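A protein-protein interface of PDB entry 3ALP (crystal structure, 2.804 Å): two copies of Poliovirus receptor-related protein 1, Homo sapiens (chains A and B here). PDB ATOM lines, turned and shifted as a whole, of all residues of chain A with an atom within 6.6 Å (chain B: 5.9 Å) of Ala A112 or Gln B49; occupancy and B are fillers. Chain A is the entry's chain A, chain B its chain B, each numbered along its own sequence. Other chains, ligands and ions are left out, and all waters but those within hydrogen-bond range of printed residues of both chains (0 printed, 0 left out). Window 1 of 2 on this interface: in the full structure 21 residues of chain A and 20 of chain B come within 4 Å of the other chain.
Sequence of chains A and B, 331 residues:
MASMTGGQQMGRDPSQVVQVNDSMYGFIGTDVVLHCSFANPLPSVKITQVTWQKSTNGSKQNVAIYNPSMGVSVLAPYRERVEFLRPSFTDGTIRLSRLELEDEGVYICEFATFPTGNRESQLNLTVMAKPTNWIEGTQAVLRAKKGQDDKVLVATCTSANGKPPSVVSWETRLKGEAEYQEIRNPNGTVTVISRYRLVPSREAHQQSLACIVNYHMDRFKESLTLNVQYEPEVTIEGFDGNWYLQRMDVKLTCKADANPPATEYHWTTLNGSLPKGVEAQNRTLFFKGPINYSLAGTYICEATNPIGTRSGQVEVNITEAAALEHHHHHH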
ATOM      1  N   LYS A  46      -0.245   4.069 -16.580  1.00  0.00           N
ATOM      2  CA  LYS A  46       0.207   2.867 -17.232  1.00  0.00           C
ATOM      3  C   LYS A  46       1.350   2.299 -16.433  1.00  0.00           C
ATOM      4  O   LYS A  46       2.329   2.975 -16.178  1.00  0.00           O
ATOM      5  CB  LYS A  46       0.664   3.174 -18.653  1.00  0.00           C
ATOM      6  CG  LYS A  46      -0.430   3.717 -19.542  1.00  0.00           C
ATOM      7  N   ILE A  47       1.228   1.045 -16.040  1.00  0.00           N
ATOM      8  CA  ILE A  47       2.278   0.428 -15.282  1.00  0.00           C
ATOM      9  C   ILE A  47       3.327  -0.050 -16.245  1.00  0.00           C
ATOM     10  O   ILE A  47       3.063  -0.837 -17.136  1.00  0.00           O
ATOM     11  CB  ILE A  47       1.762  -0.759 -14.494  1.00  0.00           C
ATOM     12  CG1 ILE A  47       1.040  -0.281 -13.243  1.00  0.00           C
ATOM     13  CG2 ILE A  47       2.902  -1.666 -14.124  1.00  0.00           C
ATOM     14  CD1 ILE A  47      -0.109   0.626 -13.529  1.00  0.00           C
ATOM     15  N   THR A  48       4.537   0.428 -16.031  1.00  0.00           N
ATOM     16  CA  THR A  48       5.639   0.241 -16.945  1.00  0.00           C
ATOM     17  C   THR A  48       6.443  -0.997 -16.608  1.00  0.00           C
ATOM     18  O   THR A  48       6.755  -1.788 -17.484  1.00  0.00           O
ATOM     19  CB  THR A  48       6.552   1.462 -16.859  1.00  0.00           C
ATOM     20  OG1 THR A  48       5.970   2.535 -17.605  1.00  0.00           O
ATOM     21  CG2 THR A  48       7.912   1.152 -17.408  1.00  0.00           C
ATOM     22  N   GLN A  49       6.770  -1.152 -15.327  1.00  0.00           N
ATOM     23  CA  GLN A  49       7.590  -2.261 -14.835  1.00  0.00           C
ATOM     24  C   GLN A  49       7.342  -2.485 -13.330  1.00  0.00           C
ATOM     25  O   GLN A  49       6.974  -1.556 -12.619  1.00  0.00           O
ATOM     26  CB  GLN A  49       9.063  -1.947 -15.096  1.00  0.00           C
ATOM     27  CG  GLN A  49      10.038  -3.044 -14.765  1.00  0.00           C
ATOM     28  CD  GLN A  49      11.393  -2.777 -15.394  1.00  0.00           C
ATOM     29  OE1 GLN A  49      11.484  -2.529 -16.591  1.00  0.00           O
ATOM     30  NE2 GLN A  49      12.448  -2.820 -14.593  1.00  0.00           N
ATOM     31  N   VAL A  50       7.528  -3.715 -12.856  1.00  0.00           N
ATOM     32  CA  VAL A  50       7.436  -4.022 -11.426  1.00  0.00           C
ATOM     33  C   VAL A  50       8.726  -4.659 -10.932  1.00  0.00           C
ATOM     34  O   VAL A  50       9.183  -5.638 -11.500  1.00  0.00           O
ATOM     35  CB  VAL A  50       6.288  -4.982 -11.142  1.00  0.00           C
ATOM     36  CG1 VAL A  50       6.372  -5.469  -9.758  1.00  0.00           C
ATOM     37  CG2 VAL A  50       4.980  -4.282 -11.347  1.00  0.00           C
ATOM     38  N   THR A  51       9.311  -4.112  -9.872  1.00  0.00           N
ATOM     39  CA  THR A  51      10.658  -4.501  -9.458  1.00  0.00           C
ATOM     40  C   THR A  51      10.806  -4.784  -7.962  1.00  0.00           C
ATOM     41  O   THR A  51      10.433  -3.955  -7.136  1.00  0.00           O
ATOM     42  CB  THR A  51      11.672  -3.396  -9.825  1.00  0.00           C
ATOM     43  OG1 THR A  51      11.663  -3.188 -11.240  1.00  0.00           O
ATOM     44  CG2 THR A  51      13.064  -3.784  -9.394  1.00  0.00           C
ATOM     45  N   GLU A 110       8.629  -2.025  -6.130  1.00  0.00           N
ATOM     46  CA  GLU A 110       8.354  -0.751  -6.765  1.00  0.00           C
ATOM     47  C   GLU A 110       7.588  -0.907  -8.073  1.00  0.00           C
ATOM     48  O   GLU A 110       7.991  -1.664  -8.941  1.00  0.00           O
ATOM     49  CB  GLU A 110       9.666  -0.021  -7.010  1.00  0.00           C
ATOM     50  CG  GLU A 110       9.634   0.969  -8.136  1.00  0.00           C
ATOM     51  CD  GLU A 110      11.016   1.444  -8.479  1.00  0.00           C
ATOM     52  OE1 GLU A 110      11.352   1.523  -9.691  1.00  0.00           O
ATOM     53  OE2 GLU A 110      11.770   1.710  -7.520  1.00  0.00           O
ATOM     54  N   PHE A 111       6.471  -0.195  -8.190  1.00  0.00           N
ATOM     55  CA  PHE A 111       5.728  -0.101  -9.436  1.00  0.00           C
ATOM     56  C   PHE A 111       6.128   1.154 -10.180  1.00  0.00           C
ATOM     57  O   PHE A 111       5.749   2.250  -9.766  1.00  0.00           O
ATOM     58  CB  PHE A 111       4.233   0.007  -9.162  1.00  0.00           C
ATOM     59  CG  PHE A 111       3.584  -1.293  -8.887  1.00  0.00           C
ATOM     60  CD1 PHE A 111       2.888  -1.945  -9.870  1.00  0.00           C
ATOM     61  CD2 PHE A 111       3.671  -1.872  -7.640  1.00  0.00           C
ATOM     62  CE1 PHE A 111       2.293  -3.163  -9.610  1.00  0.00           C
ATOM     63  CE2 PHE A 111       3.074  -3.087  -7.380  1.00  0.00           C
ATOM     64  CZ  PHE A 111       2.392  -3.733  -8.361  1.00  0.00           C
ATOM     65  N   ALA A 112       6.871   1.002 -11.276  1.00  0.00           N
ATOM     66  CA  ALA A 112       7.163   2.127 -12.167  1.00  0.00           C
ATOM     67  C   ALA A 112       5.963   2.421 -13.059  1.00  0.00           C
ATOM     68  O   ALA A 112       5.475   1.533 -13.756  1.00  0.00           O
ATOM     69  CB  ALA A 112       8.365   1.832 -13.012  1.00  0.00           C
ATOM     70  N   THR A 113       5.483   3.661 -13.038  1.00  0.00           N
ATOM     71  CA  THR A 113       4.298   4.006 -13.812  1.00  0.00           C
ATOM     72  C   THR A 113       4.471   5.308 -14.559  1.00  0.00           C
ATOM     73  O   THR A 113       5.291   6.147 -14.194  1.00  0.00           O
ATOM     74  CB  THR A 113       3.069   4.187 -12.926  1.00  0.00           C
ATOM     75  OG1 THR A 113       3.057   5.524 -12.413  1.00  0.00           O
ATOM     76  CG2 THR A 113       3.066   3.195 -11.784  1.00  0.00           C
ATOM     77  N   PHE A 114       3.669   5.477 -15.600  1.00  0.00           N
ATOM     78  CA  PHE A 114       3.703   6.686 -16.403  1.00  0.00           C
ATOM     79  C   PHE A 114       2.275   7.173 -16.606  1.00  0.00           C
ATOM     80  O   PHE A 114       1.380   6.374 -16.883  1.00  0.00           O
ATOM     81  CB  PHE A 114       4.374   6.410 -17.745  1.00  0.00           C
ATOM     82  CG  PHE A 114       4.750   7.645 -18.492  1.00  0.00           C
ATOM     83  CD1 PHE A 114       6.071   8.032 -18.595  1.00  0.00           C
ATOM     84  CD2 PHE A 114       3.787   8.425 -19.095  1.00  0.00           C
ATOM     85  CE1 PHE A 114       6.425   9.179 -19.287  1.00  0.00           C
ATOM     86  CE2 PHE A 114       4.135   9.566 -19.786  1.00  0.00           C
ATOM     87  CZ  PHE A 114       5.454   9.946 -19.881  1.00  0.00           C
ATOM     88  N   GLY A 117       4.889   8.351 -12.169  1.00  0.00           N
ATOM     89  CA  GLY A 117       6.123   7.997 -11.487  1.00  0.00           C
ATOM     90  C   GLY A 117       6.040   6.737 -10.644  1.00  0.00           C
ATOM     91  O   GLY A 117       5.110   5.950 -10.776  1.00  0.00           O
ATOM     92  N   ASN A 118       7.007   6.550  -9.753  1.00  0.00           N
ATOM     93  CA  ASN A 118       7.137   5.288  -9.026  1.00  0.00           C
ATOM     94  C   ASN A 118       6.348   5.247  -7.729  1.00  0.00           C
ATOM     95  O   ASN A 118       6.182   6.265  -7.055  1.00  0.00           O
ATOM     96  CB  ASN A 118       8.616   4.927  -8.787  1.00  0.00           C
ATOM     97  CG  ASN A 118       9.421   4.800 -10.090  1.00  0.00           C
ATOM     98  OD1 ASN A 118       8.974   5.206 -11.183  1.00  0.00           O
ATOM     99  ND2 ASN A 118      10.620   4.244  -9.975  1.00  0.00           N
ATOM    100  N   ARG A 119       5.862   4.053  -7.398  1.00  0.00           N
ATOM    101  CA  ARG A 119       5.097   3.802  -6.182  1.00  0.00           C
ATOM    102  C   ARG A 119       5.672   2.565  -5.512  1.00  0.00           C
ATOM    103  O   ARG A 119       5.690   1.496  -6.107  1.00  0.00           O
ATOM    104  CB  ARG A 119       3.623   3.563  -6.526  1.00  0.00           C
ATOM    105  CG  ARG A 119       2.638   4.174  -5.546  1.00  0.00           C
ATOM    106  CD  ARG A 119       2.114   3.156  -4.550  1.00  0.00           C
ATOM    107  NE  ARG A 119       0.781   2.642  -4.884  1.00  0.00           N
ATOM    108  CZ  ARG A 119      -0.202   3.344  -5.452  1.00  0.00           C
ATOM    109  NH1 ARG A 119      -0.046   4.627  -5.770  1.00  0.00           N
ATOM    110  NH2 ARG A 119      -1.365   2.752  -5.697  1.00  0.00           N
ATOM    111  N   ILE B  47      16.738   0.029 -21.395  1.00  0.00           N
ATOM    112  CA  ILE B  47      16.337   0.995 -20.389  1.00  0.00           C
ATOM    113  C   ILE B  47      14.856   1.327 -20.519  1.00  0.00           C
ATOM    114  O   ILE B  47      14.411   1.968 -21.455  1.00  0.00           O
ATOM    115  CB  ILE B  47      17.184   2.272 -20.430  1.00  0.00           C
ATOM    116  CG1 ILE B  47      18.554   2.022 -19.787  1.00  0.00           C
ATOM    117  CG2 ILE B  47      16.472   3.402 -19.710  1.00  0.00           C
ATOM    118  CD1 ILE B  47      19.510   1.197 -20.634  1.00  0.00           C
ATOM    119  N   THR B  48      14.107   0.872 -19.540  1.00  0.00           N
ATOM    120  CA  THR B  48      12.668   1.013 -19.488  1.00  0.00           C
ATOM    121  C   THR B  48      12.137   2.410 -19.109  1.00  0.00           C
ATOM    122  O   THR B  48      11.147   2.867 -19.668  1.00  0.00           O
ATOM    123  CB  THR B  48      12.165   0.023 -18.451  1.00  0.00           C
ATOM    124  OG1 THR B  48      12.425  -1.305 -18.919  1.00  0.00           O
ATOM    125  CG2 THR B  48      10.698   0.210 -18.190  1.00  0.00           C
ATOM    126  N   GLN B  49      12.767   3.081 -18.148  1.00  0.00           N
ATOM    127  CA  GLN B  49      12.231   4.345 -17.657  1.00  0.00           C
ATOM    128  C   GLN B  49      13.224   5.082 -16.740  1.00  0.00           C
ATOM    129  O   GLN B  49      13.981   4.453 -16.003  1.00  0.00           O
ATOM    130  CB  GLN B  49      10.911   4.075 -16.932  1.00  0.00           C
ATOM    131  CG  GLN B  49      10.191   5.300 -16.429  1.00  0.00           C
ATOM    132  CD  GLN B  49       8.747   5.015 -16.053  1.00  0.00           C
ATOM    133  OE1 GLN B  49       8.317   5.295 -14.936  1.00  0.00           O
ATOM    134  NE2 GLN B  49       7.990   4.456 -16.989  1.00  0.00           N
ATOM    135  N   VAL B  50      13.215   6.413 -16.792  1.00  0.00           N
ATOM    136  CA  VAL B  50      14.104   7.226 -15.964  1.00  0.00           C
ATOM    137  C   VAL B  50      13.340   8.156 -15.033  1.00  0.00           C
ATOM    138  O   VAL B  50      12.655   9.067 -15.475  1.00  0.00           O
ATOM    139  CB  VAL B  50      15.038   8.065 -16.824  1.00  0.00           C
ATOM    140  CG1 VAL B  50      15.922   8.918 -15.957  1.00  0.00           C
ATOM    141  CG2 VAL B  50      15.886   7.169 -17.670  1.00  0.00           C
ATOM    142  N   THR B  51      13.476   7.932 -13.736  1.00  0.00           N
ATOM    143  CA  THR B  51      12.643   8.619 -12.765  1.00  0.00           C
ATOM    144  C   THR B  51      13.429   9.422 -11.735  1.00  0.00           C
ATOM    145  O   THR B  51      14.270   8.875 -11.018  1.00  0.00           O
ATOM    146  CB  THR B  51      11.790   7.614 -12.010  1.00  0.00           C
ATOM    147  OG1 THR B  51      11.116   6.762 -12.944  1.00  0.00           O
ATOM    148  CG2 THR B  51      10.778   8.337 -11.166  1.00  0.00           C
ATOM    149  N   ILE B  65       9.659  12.241 -14.999  1.00  0.00           N
ATOM    150  CA  ILE B  65       9.839  10.912 -15.569  1.00  0.00           C
ATOM    151  C   ILE B  65      10.171  10.999 -17.050  1.00  0.00           C
ATOM    152  O   ILE B  65       9.673  11.862 -17.753  1.00  0.00           O
ATOM    153  CB  ILE B  65       8.575  10.034 -15.392  1.00  0.00           C
ATOM    154  CG1 ILE B  65       8.158   9.963 -13.927  1.00  0.00           C
ATOM    155  CG2 ILE B  65       8.807   8.636 -15.920  1.00  0.00           C
ATOM    156  CD1 ILE B  65       7.055  10.911 -13.578  1.00  0.00           C
ATOM    157  N   TYR B  66      11.036  10.113 -17.516  1.00  0.00           N
ATOM    158  CA  TYR B  66      11.252   9.956 -18.944  1.00  0.00           C
ATOM    159  C   TYR B  66      11.092   8.499 -19.291  1.00  0.00           C
ATOM    160  O   TYR B  66      11.734   7.632 -18.702  1.00  0.00           O
ATOM    161  CB  TYR B  66      12.635  10.440 -19.373  1.00  0.00           C
ATOM    162  CG  TYR B  66      13.009  10.051 -20.791  1.00  0.00           C
ATOM    163  CD1 TYR B  66      12.348  10.600 -21.882  1.00  0.00           C
ATOM    164  CD2 TYR B  66      14.028   9.151 -21.040  1.00  0.00           C
ATOM    165  CE1 TYR B  66      12.682  10.250 -23.177  1.00  0.00           C
ATOM    166  CE2 TYR B  66      14.375   8.795 -22.340  1.00  0.00           C
ATOM    167  CZ  TYR B  66      13.693   9.346 -23.405  1.00  0.00           C
ATOM    168  OH  TYR B  66      14.023   8.995 -24.702  1.00  0.00           O
ATOM    169  N   ASN B  67      10.193   8.236 -20.228  1.00  0.00           N
ATOM    170  CA  ASN B  67      10.004   6.906 -20.773  1.00  0.00           C
ATOM    171  C   ASN B  67      10.296   6.999 -22.255  1.00  0.00           C
ATOM    172  O   ASN B  67       9.679   7.789 -22.966  1.00  0.00           O
ATOM    173  CB  ASN B  67       8.580   6.424 -20.515  1.00  0.00           C
ATOM    174  CG  ASN B  67       8.361   5.012 -20.966  1.00  0.00           C
ATOM    175  OD1 ASN B  67       8.745   4.633 -22.068  1.00  0.00           O
ATOM    176  ND2 ASN B  67       7.733   4.217 -20.118  1.00  0.00           N
ATOM    177  N   PRO B  68      11.269   6.221 -22.725  1.00  0.00           N
ATOM    178  CA  PRO B  68      11.675   6.269 -24.131  1.00  0.00           C
ATOM    179  C   PRO B  68      10.501   6.146 -25.103  1.00  0.00           C
ATOM    180  O   PRO B  68      10.577   6.676 -26.214  1.00  0.00           O
ATOM    181  CB  PRO B  68      12.608   5.065 -24.253  1.00  0.00           C
ATOM    182  CG  PRO B  68      13.193   4.923 -22.905  1.00  0.00           C
ATOM    183  CD  PRO B  68      12.086   5.276 -21.950  1.00  0.00           C
ATOM    184  N   GLU B 110      16.596   7.307 -10.837  1.00  0.00           N
ATOM    185  CA  GLU B 110      16.521   5.861 -10.971  1.00  0.00           C
ATOM    186  C   GLU B 110      16.283   5.425 -12.403  1.00  0.00           C
ATOM    187  O   GLU B 110      15.267   5.744 -13.003  1.00  0.00           O
ATOM    188  CB  GLU B 110      15.421   5.318 -10.075  1.00  0.00           C
ATOM    189  CG  GLU B 110      15.053   3.881 -10.320  1.00  0.00           C
ATOM    190  CD  GLU B 110      14.157   3.361  -9.231  1.00  0.00           C
ATOM    191  OE1 GLU B 110      14.228   2.154  -8.917  1.00  0.00           O
ATOM    192  OE2 GLU B 110      13.401   4.180  -8.664  1.00  0.00           O
ATOM    193  N   PHE B 111      17.242   4.696 -12.947  1.00  0.00           N
ATOM    194  CA  PHE B 111      17.077   4.026 -14.225  1.00  0.00           C
ATOM    195  C   PHE B 111      16.450   2.662 -14.018  1.00  0.00           C
ATOM    196  O   PHE B 111      17.074   1.781 -13.417  1.00  0.00           O
ATOM    197  CB  PHE B 111      18.440   3.835 -14.895  1.00  0.00           C
ATOM    198  CG  PHE B 111      18.918   5.041 -15.651  1.00  0.00           C
ATOM    199  CD1 PHE B 111      18.713   5.147 -17.009  1.00  0.00           C
ATOM    200  CD2 PHE B 111      19.574   6.059 -15.010  1.00  0.00           C
ATOM    201  CE1 PHE B 111      19.151   6.248 -17.702  1.00  0.00           C
ATOM    202  CE2 PHE B 111      20.003   7.159 -15.703  1.00  0.00           C
ATOM    203  CZ  PHE B 111      19.786   7.253 -17.049  1.00  0.00           C
ATOM    204  N   ALA B 112      15.218   2.493 -14.496  1.00  0.00           N
ATOM    205  CA  ALA B 112      14.594   1.167 -14.567  1.00  0.00           C
ATOM    206  C   ALA B 112      15.017   0.452 -15.843  1.00  0.00           C
ATOM    207  O   ALA B 112      14.765   0.933 -16.940  1.00  0.00           O
ATOM    208  CB  ALA B 112      13.092   1.279 -14.534  1.00  0.00           C
ATOM    209  N   THR B 113      15.656  -0.700 -15.704  1.00  0.00           N
ATOM    210  CA  THR B 113      16.025  -1.466 -16.883  1.00  0.00           C
ATOM    211  C   THR B 113      15.449  -2.871 -16.810  1.00  0.00           C
ATOM    212  O   THR B 113      15.024  -3.322 -15.742  1.00  0.00           O
ATOM    213  CB  THR B 113      17.538  -1.583 -17.021  1.00  0.00           C
ATOM    214  OG1 THR B 113      17.998  -2.708 -16.263  1.00  0.00           O
ATOM    215  CG2 THR B 113      18.216  -0.327 -16.528  1.00  0.00           C
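Of the printed residues of chain B, Glu A110 touches Glu B110. Of the printed residues of chain A, Thr B48 touches Thr A48 and Gln A49. Of chain A, only Thr A48 (2.9 Å), Ala A112 (3.96 Å), Thr A113 (3.2 Å) and Asn A118 (3.8 Å) come within 4 Å of Gln B49. Printed residues of chain A within 4 Å of Asn B67: Thr A48 (3.5 Å) and Phe A114 (3.5 Å). Of the printed residues of chain A, Glu B110 touches Glu A110 (2.9 Å) and Asn A118 (3.1 Å). Ala B112 touches none of the printed residues of chain A. The nearest residue of chain A that does not touch Gln B49 is Phe A114 (4.2 Å). The nearest printed residue of chain A that does not touch Ile B65 is Thr A113 (4.6 Å).
Of the 13 printed residues of chain B, 7 touch a printed residue of chain A. Hydrophobic or aromatic side chains of chain B within 4 Å of the printed part of chain A: Ile B65. Hydrophobic or aromatic side chains of chain A within 4 Å of the printed part of chain B: Ala A112 and Phe A114.
Thr A48 touches its own counterpart, Thr B48. Gln A49 touches Thr B113, and with the chains exchanged Thr A113 touches Gln B49. Glu B110 touches its own counterpart, Glu A110. Ala A112 touches Gln B49, but with the chains exchanged Gln A49 does not touch Ala B112 (4.1 Å). 9 positions are printed for both chains.
N of Thr A48 is in hydrogen-bond range of O of Ala A112. NE2 of Gln A49 sits at hydrogen-bond distance from OG1 of Thr A51 (3.5 Å). The backbone carbonyl oxygen (O) of Ala B112 is in hydrogen-bond range of the backbone NH (N) of Thr B48. N of Glu A110 lies within hydrogen-bond range of O of Thr A51 (2.8 Å). O of Gly A117 lies within hydrogen-bond range of OG1 of Thr A113 (2.7 Å). N of Lys A46 sits at hydrogen-bond distance from O of Phe A114 (2.8 Å).
The side-chain hydroxyl (OG1) of Thr A48 is in hydrogen-bond range of the side-chain amide nitrogen (NE2) of Gln B49, at 2.9 Å. The side-chain carboxylate (OE2) of Glu B110 sits at hydrogen-bond distance from the side-chain amide nitrogen (ND2) of Asn A118 (3.1 Å). OE1 of Gln A49 sits at hydrogen-bond distance from OG1 of Thr B48. The side-chain amide nitrogen (NE2) of Gln A49 is in hydrogen-bond range of the backbone carbonyl oxygen (O) of Thr B113 (2.9 Å). OD1 of Asn A118 sits at hydrogen-bond distance from OG1 of Thr B51, 3.2 Å away. The backbone carbonyl oxygen (O) of Thr A113 sits close to the side-chain amide oxygen (OE1) of Gln B49 (3.2 Å). OE1 of Glu B110 sits close to OE2 of Glu A110 (2.9 Å).
Among the printed residues, merely in contact across the chains: Thr A48 with Thr B48 (3.0 Å), Thr A48 with Asn B67 (3.5 Å), Phe A114 with Asn B67 (3.5 Å), Gly A117 with Ile B65 (3.6 Å), Asn A118 with Gln B49 (3.8 Å), Phe A114 with Ile B65 (3.9 Å) and Ala A112 with Gln B49 (3.96 Å).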
